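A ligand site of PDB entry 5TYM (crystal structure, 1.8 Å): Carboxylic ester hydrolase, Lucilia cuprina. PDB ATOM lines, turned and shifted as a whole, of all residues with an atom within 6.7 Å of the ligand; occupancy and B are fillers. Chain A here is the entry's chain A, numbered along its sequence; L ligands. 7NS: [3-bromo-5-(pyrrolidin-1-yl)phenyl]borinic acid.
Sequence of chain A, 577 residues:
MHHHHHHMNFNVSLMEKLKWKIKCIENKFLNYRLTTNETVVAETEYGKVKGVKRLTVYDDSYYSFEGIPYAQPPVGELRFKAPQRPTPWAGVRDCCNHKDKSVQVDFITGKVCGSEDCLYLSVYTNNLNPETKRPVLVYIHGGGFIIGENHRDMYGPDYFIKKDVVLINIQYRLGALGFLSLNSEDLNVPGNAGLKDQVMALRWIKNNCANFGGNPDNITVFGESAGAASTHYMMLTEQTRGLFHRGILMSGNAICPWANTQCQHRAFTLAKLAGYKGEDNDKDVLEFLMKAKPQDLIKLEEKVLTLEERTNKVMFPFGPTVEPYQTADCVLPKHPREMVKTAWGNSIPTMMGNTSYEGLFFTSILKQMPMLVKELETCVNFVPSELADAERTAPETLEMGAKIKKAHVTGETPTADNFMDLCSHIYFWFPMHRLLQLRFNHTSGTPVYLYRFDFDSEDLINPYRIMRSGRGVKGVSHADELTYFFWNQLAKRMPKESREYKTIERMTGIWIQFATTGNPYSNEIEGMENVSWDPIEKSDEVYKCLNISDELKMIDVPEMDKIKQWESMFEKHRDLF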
ATOM      1  N   HIS A 141      10.352  -0.812  -4.847  1.00  0.00           N
ATOM      2  CA  HIS A 141      11.329  -1.461  -5.708  1.00  0.00           C
ATOM      3  C   HIS A 141      12.775  -1.150  -5.314  1.00  0.00           C
ATOM      4  O   HIS A 141      13.071  -0.117  -4.713  1.00  0.00           O
ATOM      5  CB  HIS A 141      11.078  -1.066  -7.177  1.00  0.00           C
ATOM      6  CG  HIS A 141      11.458   0.343  -7.514  1.00  0.00           C
ATOM      7  ND1 HIS A 141      12.766   0.740  -7.705  1.00  0.00           N
ATOM      8  CD2 HIS A 141      10.706   1.449  -7.725  1.00  0.00           C
ATOM      9  CE1 HIS A 141      12.803   2.025  -8.000  1.00  0.00           C
ATOM     10  NE2 HIS A 141      11.564   2.486  -8.006  1.00  0.00           N
ATOM     11  N   GLY A 142      13.661  -2.091  -5.632  1.00  0.00           N
ATOM     12  CA  GLY A 142      15.093  -1.897  -5.507  1.00  0.00           C
ATOM     13  C   GLY A 142      15.726  -1.365  -6.796  1.00  0.00           C
ATOM     14  O   GLY A 142      15.010  -0.873  -7.681  1.00  0.00           O
ATOM     15  N   GLY A 143      17.041  -1.508  -6.901  1.00  0.00           N
ATOM     16  CA  GLY A 143      17.827  -0.969  -8.005  1.00  0.00           C
ATOM     17  C   GLY A 143      18.868   0.034  -7.509  1.00  0.00           C
ATOM     18  O   GLY A 143      19.163   1.041  -8.183  1.00  0.00           O
ATOM     19  N   GLY A 144      19.406  -0.212  -6.308  1.00  0.00           N
ATOM     20  CA  GLY A 144      20.544   0.546  -5.817  1.00  0.00           C
ATOM     21  C   GLY A 144      20.319   2.034  -5.612  1.00  0.00           C
ATOM     22  O   GLY A 144      21.265   2.805  -5.481  1.00  0.00           O
ATOM     23  N   PHE A 145      19.054   2.421  -5.534  1.00  0.00           N
ATOM     24  CA  PHE A 145      18.617   3.818  -5.454  1.00  0.00           C
ATOM     25  C   PHE A 145      18.965   4.621  -6.721  1.00  0.00           C
ATOM     26  O   PHE A 145      18.895   5.857  -6.697  1.00  0.00           O
ATOM     27  CB  PHE A 145      19.221   4.547  -4.249  1.00  0.00           C
ATOM     28  CG  PHE A 145      18.866   3.916  -2.939  1.00  0.00           C
ATOM     29  CD1 PHE A 145      17.653   4.180  -2.338  1.00  0.00           C
ATOM     30  CD2 PHE A 145      19.762   3.074  -2.317  1.00  0.00           C
ATOM     31  CE1 PHE A 145      17.319   3.596  -1.123  1.00  0.00           C
ATOM     32  CE2 PHE A 145      19.433   2.469  -1.094  1.00  0.00           C
ATOM     33  CZ  PHE A 145      18.220   2.741  -0.500  1.00  0.00           C
ATOM     34  N   ILE A 146      19.332   3.908  -7.782  1.00  0.00           N
ATOM     35  CA  ILE A 146      19.674   4.546  -9.043  1.00  0.00           C
ATOM     36  C   ILE A 146      18.856   4.070 -10.260  1.00  0.00           C
ATOM     37  O   ILE A 146      18.796   4.777 -11.288  1.00  0.00           O
ATOM     38  CB  ILE A 146      21.185   4.353  -9.371  1.00  0.00           C
ATOM     39  CG1 ILE A 146      21.539   2.875  -9.500  1.00  0.00           C
ATOM     40  CG2 ILE A 146      22.044   5.018  -8.320  1.00  0.00           C
ATOM     41  CD1 ILE A 146      22.932   2.657 -10.047  1.00  0.00           C
ATOM     42  N   ILE A 147      18.237   2.896 -10.177  1.00  0.00           N
ATOM     43  CA  ILE A 147      17.311   2.443 -11.229  1.00  0.00           C
ATOM     44  C   ILE A 147      16.029   1.902 -10.619  1.00  0.00           C
ATOM     45  O   ILE A 147      15.962   1.700  -9.399  1.00  0.00           O
ATOM     46  CB  ILE A 147      17.926   1.349 -12.138  1.00  0.00           C
ATOM     47  CG1 ILE A 147      18.387   0.141 -11.303  1.00  0.00           C
ATOM     48  CG2 ILE A 147      19.062   1.924 -13.019  1.00  0.00           C
ATOM     49  CD1 ILE A 147      18.782  -1.077 -12.175  1.00  0.00           C
ATOM     50  N   GLU A 224      12.588  -5.211  -2.148  1.00  0.00           N
ATOM     51  CA  GLU A 224      13.778  -6.030  -2.339  1.00  0.00           C
ATOM     52  C   GLU A 224      14.979  -5.123  -2.630  1.00  0.00           C
ATOM     53  O   GLU A 224      14.835  -4.113  -3.344  1.00  0.00           O
ATOM     54  CB  GLU A 224      13.574  -7.019  -3.488  1.00  0.00           C
ATOM     55  CG  GLU A 224      14.664  -8.041  -3.638  1.00  0.00           C
ATOM     56  CD  GLU A 224      15.652  -7.684  -4.729  1.00  0.00           C
ATOM     57  OE1 GLU A 224      15.394  -6.676  -5.429  1.00  0.00           O
ATOM     58  OE2 GLU A 224      16.674  -8.380  -4.893  1.00  0.00           O
ATOM     59  N   SER A 225      16.148  -5.479  -2.100  1.00  0.00           N
ATOM     60  CA  SER A 225      17.393  -4.767  -2.358  1.00  0.00           C
ATOM     61  C   SER A 225      17.285  -3.336  -1.819  1.00  0.00           C
ATOM     62  O   SER A 225      17.012  -3.152  -0.636  1.00  0.00           O
ATOM     63  CB  SER A 225      17.710  -4.792  -3.863  1.00  0.00           C
ATOM     64  OG  SER A 225      19.106  -4.748  -4.110  1.00  0.00           O
ATOM     65  N   ALA A 226      17.486  -2.309  -2.652  1.00  0.00           N
ATOM     66  CA  ALA A 226      17.325  -0.939  -2.171  1.00  0.00           C
ATOM     67  C   ALA A 226      15.887  -0.651  -1.682  1.00  0.00           C
ATOM     68  O   ALA A 226      15.702   0.193  -0.819  1.00  0.00           O
ATOM     69  CB  ALA A 226      17.735   0.057  -3.250  1.00  0.00           C
ATOM     70  N   GLY A 227      14.910  -1.393  -2.175  1.00  0.00           N
ATOM     71  CA  GLY A 227      13.574  -1.378  -1.592  1.00  0.00           C
ATOM     72  C   GLY A 227      13.488  -2.007  -0.188  1.00  0.00           C
ATOM     73  O   GLY A 227      12.604  -1.663   0.608  1.00  0.00           O
ATOM     74  N   ALA A 228      14.379  -2.935   0.110  1.00  0.00           N
ATOM     75  CA  ALA A 228      14.459  -3.520   1.441  1.00  0.00           C
ATOM     76  C   ALA A 228      15.117  -2.533   2.407  1.00  0.00           C
ATOM     77  O   ALA A 228      14.603  -2.255   3.493  1.00  0.00           O
ATOM     78  CB  ALA A 228      15.240  -4.830   1.409  1.00  0.00           C
ATOM     79  N   SER A 251      16.344  -9.235   1.033  1.00  0.00           N
ATOM     80  CA  SER A 251      17.744  -9.066   0.615  1.00  0.00           C
ATOM     81  C   SER A 251      18.266  -7.646   0.805  1.00  0.00           C
ATOM     82  O   SER A 251      18.807  -7.055  -0.157  1.00  0.00           O
ATOM     83  CB  SER A 251      17.956  -9.415  -0.868  1.00  0.00           C
ATOM     84  OG  SER A 251      17.526 -10.720  -1.172  1.00  0.00           O
ATOM     85  N   TRP A 258      26.171  -0.689   1.317  1.00  0.00           N
ATOM     86  CA  TRP A 258      25.805  -0.079   0.033  1.00  0.00           C
ATOM     87  C   TRP A 258      24.559   0.804   0.176  1.00  0.00           C
ATOM     88  O   TRP A 258      24.179   1.487  -0.755  1.00  0.00           O
ATOM     89  CB  TRP A 258      25.579  -1.164  -1.041  1.00  0.00           C
ATOM     90  CG  TRP A 258      24.582  -2.238  -0.598  1.00  0.00           C
ATOM     91  CD1 TRP A 258      24.875  -3.461  -0.040  1.00  0.00           C
ATOM     92  CD2 TRP A 258      23.160  -2.167  -0.658  1.00  0.00           C
ATOM     93  NE1 TRP A 258      23.714  -4.140   0.263  1.00  0.00           N
ATOM     94  CE2 TRP A 258      22.643  -3.377  -0.123  1.00  0.00           C
ATOM     95  CE3 TRP A 258      22.255  -1.198  -1.127  1.00  0.00           C
ATOM     96  CZ2 TRP A 258      21.288  -3.634  -0.031  1.00  0.00           C
ATOM     97  CZ3 TRP A 258      20.900  -1.455  -1.035  1.00  0.00           C
ATOM     98  CH2 TRP A 258      20.427  -2.675  -0.482  1.00  0.00           C
ATOM     99  N   MET A 315      29.606   1.745  -3.324  1.00  0.00           N
ATOM    100  CA  MET A 315      28.874   1.207  -4.450  1.00  0.00           C
ATOM    101  C   MET A 315      28.302   2.298  -5.339  1.00  0.00           C
ATOM    102  O   MET A 315      28.358   2.201  -6.558  1.00  0.00           O
ATOM    103  CB  MET A 315      27.780   0.297  -3.940  1.00  0.00           C
ATOM    104  CG  MET A 315      28.291  -1.088  -3.744  1.00  0.00           C
ATOM    105  SD  MET A 315      28.302  -1.856  -5.369  1.00  0.00           S
ATOM    106  CE  MET A 315      26.548  -1.915  -5.590  1.00  0.00           C
ATOM    107  N   PHE A 316      27.745   3.323  -4.697  1.00  0.00           N
ATOM    108  CA  PHE A 316      27.076   4.403  -5.412  1.00  0.00           C
ATOM    109  C   PHE A 316      27.506   5.769  -4.881  1.00  0.00           C
ATOM    110  O   PHE A 316      27.677   5.957  -3.677  1.00  0.00           O
ATOM    111  CB  PHE A 316      25.548   4.275  -5.287  1.00  0.00           C
ATOM    112  CG  PHE A 316      25.014   2.876  -5.526  1.00  0.00           C
ATOM    113  CD1 PHE A 316      24.770   2.399  -6.816  1.00  0.00           C
ATOM    114  CD2 PHE A 316      24.685   2.063  -4.451  1.00  0.00           C
ATOM    115  CE1 PHE A 316      24.241   1.106  -7.020  1.00  0.00           C
ATOM    116  CE2 PHE A 316      24.162   0.797  -4.643  1.00  0.00           C
ATOM    117  CZ  PHE A 316      23.943   0.318  -5.907  1.00  0.00           C
ATOM    118  N   PHE A 361      24.871 -12.201  -8.403  1.00  0.00           N
ATOM    119  CA  PHE A 361      24.419 -10.931  -8.952  1.00  0.00           C
ATOM    120  C   PHE A 361      25.557 -10.120  -9.559  1.00  0.00           C
ATOM    121  O   PHE A 361      25.337  -9.257 -10.402  1.00  0.00           O
ATOM    122  CB  PHE A 361      23.739 -10.149  -7.829  1.00  0.00           C
ATOM    123  CG  PHE A 361      23.037  -8.886  -8.266  1.00  0.00           C
ATOM    124  CD1 PHE A 361      21.876  -8.951  -9.028  1.00  0.00           C
ATOM    125  CD2 PHE A 361      23.483  -7.656  -7.840  1.00  0.00           C
ATOM    126  CE1 PHE A 361      21.198  -7.817  -9.382  1.00  0.00           C
ATOM    127  CE2 PHE A 361      22.817  -6.487  -8.202  1.00  0.00           C
ATOM    128  CZ  PHE A 361      21.673  -6.576  -8.975  1.00  0.00           C
ATOM    129  N   PHE A 362      26.777 -10.378  -9.116  1.00  0.00           N
ATOM    130  CA  PHE A 362      27.910  -9.577  -9.565  1.00  0.00           C
ATOM    131  C   PHE A 362      28.707 -10.223 -10.698  1.00  0.00           C
ATOM    132  O   PHE A 362      29.801  -9.762 -11.017  1.00  0.00           O
ATOM    133  CB  PHE A 362      28.822  -9.265  -8.385  1.00  0.00           C
ATOM    134  CG  PHE A 362      28.128  -8.478  -7.314  1.00  0.00           C
ATOM    135  CD1 PHE A 362      27.965  -7.104  -7.445  1.00  0.00           C
ATOM    136  CD2 PHE A 362      27.603  -9.118  -6.204  1.00  0.00           C
ATOM    137  CE1 PHE A 362      27.297  -6.384  -6.468  1.00  0.00           C
ATOM    138  CE2 PHE A 362      26.936  -8.398  -5.226  1.00  0.00           C
ATOM    139  CZ  PHE A 362      26.786  -7.026  -5.360  1.00  0.00           C
ATOM    140  N   ILE A 365      29.854  -7.903 -13.538  1.00  0.00           N
ATOM    141  CA  ILE A 365      30.904  -6.994 -13.094  1.00  0.00           C
ATOM    142  C   ILE A 365      32.233  -7.726 -13.021  1.00  0.00           C
ATOM    143  O   ILE A 365      33.261  -7.196 -13.453  1.00  0.00           O
ATOM    144  CB  ILE A 365      30.551  -6.363 -11.735  1.00  0.00           C
ATOM    145  CG1 ILE A 365      29.208  -5.640 -11.845  1.00  0.00           C
ATOM    146  CG2 ILE A 365      31.648  -5.425 -11.292  1.00  0.00           C
ATOM    147  CD1 ILE A 365      29.062  -4.462 -10.922  1.00  0.00           C
ATOM    148  N   TYR A 427      27.511  -7.960   1.610  1.00  0.00           N
ATOM    149  CA  TYR A 427      26.406  -7.080   1.228  1.00  0.00           C
ATOM    150  C   TYR A 427      25.046  -7.501   1.749  1.00  0.00           C
ATOM    151  O   TYR A 427      24.128  -6.678   1.783  1.00  0.00           O
ATOM    152  CB  TYR A 427      26.346  -6.985  -0.289  1.00  0.00           C
ATOM    153  CG  TYR A 427      27.584  -6.337  -0.862  1.00  0.00           C
ATOM    154  CD1 TYR A 427      28.118  -5.177  -0.285  1.00  0.00           C
ATOM    155  CD2 TYR A 427      28.234  -6.882  -1.962  1.00  0.00           C
ATOM    156  CE1 TYR A 427      29.265  -4.571  -0.799  1.00  0.00           C
ATOM    157  CE2 TYR A 427      29.371  -6.289  -2.490  1.00  0.00           C
ATOM    158  CZ  TYR A 427      29.888  -5.152  -1.905  1.00  0.00           C
ATOM    159  OH  TYR A 427      31.010  -4.590  -2.449  1.00  0.00           O
ATOM    160  N   PHE A 428      24.907  -8.758   2.158  1.00  0.00           N
ATOM    161  CA  PHE A 428      23.579  -9.211   2.589  1.00  0.00           C
ATOM    162  C   PHE A 428      23.559  -9.924   3.936  1.00  0.00           C
ATOM    163  O   PHE A 428      22.964  -9.409   4.865  1.00  0.00           O
ATOM    164  CB  PHE A 428      22.973 -10.073   1.479  1.00  0.00           C
ATOM    165  CG  PHE A 428      22.858  -9.320   0.202  1.00  0.00           C
ATOM    166  CD1 PHE A 428      21.897  -8.352   0.071  1.00  0.00           C
ATOM    167  CD2 PHE A 428      23.744  -9.528  -0.826  1.00  0.00           C
ATOM    168  CE1 PHE A 428      21.804  -7.619  -1.099  1.00  0.00           C
ATOM    169  CE2 PHE A 428      23.643  -8.806  -1.992  1.00  0.00           C
ATOM    170  CZ  PHE A 428      22.674  -7.850  -2.120  1.00  0.00           C
ATOM    171  N   TYR A 464      16.349  -8.808 -14.461  1.00  0.00           N
ATOM    172  CA  TYR A 464      17.582  -8.756 -13.686  1.00  0.00           C
ATOM    173  C   TYR A 464      18.566  -9.868 -14.117  1.00  0.00           C
ATOM    174  O   TYR A 464      19.785  -9.658 -14.069  1.00  0.00           O
ATOM    175  CB  TYR A 464      17.298  -8.859 -12.195  1.00  0.00           C
ATOM    176  CG  TYR A 464      17.063  -7.518 -11.516  1.00  0.00           C
ATOM    177  CD1 TYR A 464      18.034  -6.525 -11.548  1.00  0.00           C
ATOM    178  CD2 TYR A 464      15.867  -7.254 -10.847  1.00  0.00           C
ATOM    179  CE1 TYR A 464      17.838  -5.298 -10.940  1.00  0.00           C
ATOM    180  CE2 TYR A 464      15.646  -6.020 -10.218  1.00  0.00           C
ATOM    181  CZ  TYR A 464      16.648  -5.047 -10.269  1.00  0.00           C
ATOM    182  OH  TYR A 464      16.451  -3.813  -9.668  1.00  0.00           O
ATOM    183  N   MET A 467      20.852  -8.644 -16.818  1.00  0.00           N
ATOM    184  CA  MET A 467      21.792  -7.601 -16.406  1.00  0.00           C
ATOM    185  C   MET A 467      23.046  -8.212 -15.764  1.00  0.00           C
ATOM    186  O   MET A 467      24.154  -7.671 -15.879  1.00  0.00           O
ATOM    187  CB  MET A 467      21.088  -6.635 -15.453  1.00  0.00           C
ATOM    188  CG  MET A 467      21.887  -5.391 -15.051  1.00  0.00           C
ATOM    189  SD  MET A 467      21.093  -4.482 -13.703  1.00  0.00           S
ATOM    190  CE  MET A 467      21.680  -5.385 -12.277  1.00  0.00           C
ATOM    191  N   HIS A 478      20.683 -12.920  -6.096  1.00  0.00           N
ATOM    192  CA  HIS A 478      19.988 -11.691  -5.767  1.00  0.00           C
ATOM    193  C   HIS A 478      18.957 -11.358  -6.871  1.00  0.00           C
ATOM    194  O   HIS A 478      19.272 -11.363  -8.076  1.00  0.00           O
ATOM    195  CB  HIS A 478      21.017 -10.547  -5.609  1.00  0.00           C
ATOM    196  CG  HIS A 478      20.484  -9.283  -5.012  1.00  0.00           C
ATOM    197  ND1 HIS A 478      20.059  -9.200  -3.700  1.00  0.00           N
ATOM    198  CD2 HIS A 478      20.366  -8.041  -5.528  1.00  0.00           C
ATOM    199  CE1 HIS A 478      19.671  -7.960  -3.453  1.00  0.00           C
ATOM    200  NE2 HIS A 478      19.870  -7.230  -4.549  1.00  0.00           N
HETATM  201 BR   7NS L   1      24.668  -4.474  -3.582  1.00  0.00          BR
HETATM  202  C02 7NS L   1      23.316  -3.900  -4.819  1.00  0.00           C
HETATM  203  C03 7NS L   1      22.003  -3.953  -4.401  1.00  0.00           C
HETATM  204  C04 7NS L   1      21.019  -3.531  -5.279  1.00  0.00           C
HETATM  205  B05 7NS L   1      19.480  -3.604  -4.763  1.00  0.00           B
HETATM  206  O06 7NS L   1      18.570  -2.537  -4.980  1.00  0.00           O
HETATM  207  C08 7NS L   1      21.289  -3.067  -6.568  1.00  0.00           C
HETATM  208  C09 7NS L   1      22.608  -3.034  -6.978  1.00  0.00           C
HETATM  209  N10 7NS L   1      22.931  -2.580  -8.293  1.00  0.00           N
HETATM  210  C11 7NS L   1      24.121  -2.642  -8.848  1.00  0.00           C
HETATM  211  C12 7NS L   1      24.040  -1.800 -10.164  1.00  0.00           C
HETATM  212  C13 7NS L   1      22.572  -1.416 -10.323  1.00  0.00           C
HETATM  213  C14 7NS L   1      21.906  -2.220  -9.469  1.00  0.00           C
HETATM  214  C15 7NS L   1      23.612  -3.463  -6.108  1.00  0.00           C
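A ring nitrogen (NE2) of His 478 lies within hydrogen-bond range of the side-chain hydroxyl of Ser 225, 2.6 Å away. N of Gly 142 lies close to O of Glu 224. NE2 of His 478 lies close to OE2 of Glu 224 (3.4 Å). The indole nitrogen (NE1) of Trp 258 lies within hydrogen-bond range of the backbone carbonyl oxygen (O) of Tyr 427, at 3.0 Å.
The side-chain hydroxyl of Ser 225 is bonded to a boron (B05) of the ligand, 1.4 Å away. O06 of the ligand sits at hydrogen-bond distance from N of Ala 226, at 2.6 Å. An oxygen (O06) of the ligand sits at hydrogen-bond distance from the backbone NH (N) of Gly 143 (2.7 Å). N of Gly 144 sits at hydrogen-bond distance from O06 of the ligand (2.8 Å).
Residues that only touch the ligand: Gly 142, Trp 258, Met 315, Phe 316, Phe 361, Phe 362 and His 478. Within 4 Å of the ligand: Gly 142, Gly 143, Gly 144, Ser 225, Ala 226, Trp 258, Met 315, Phe 316, Phe 361, Phe 362 and His 478.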
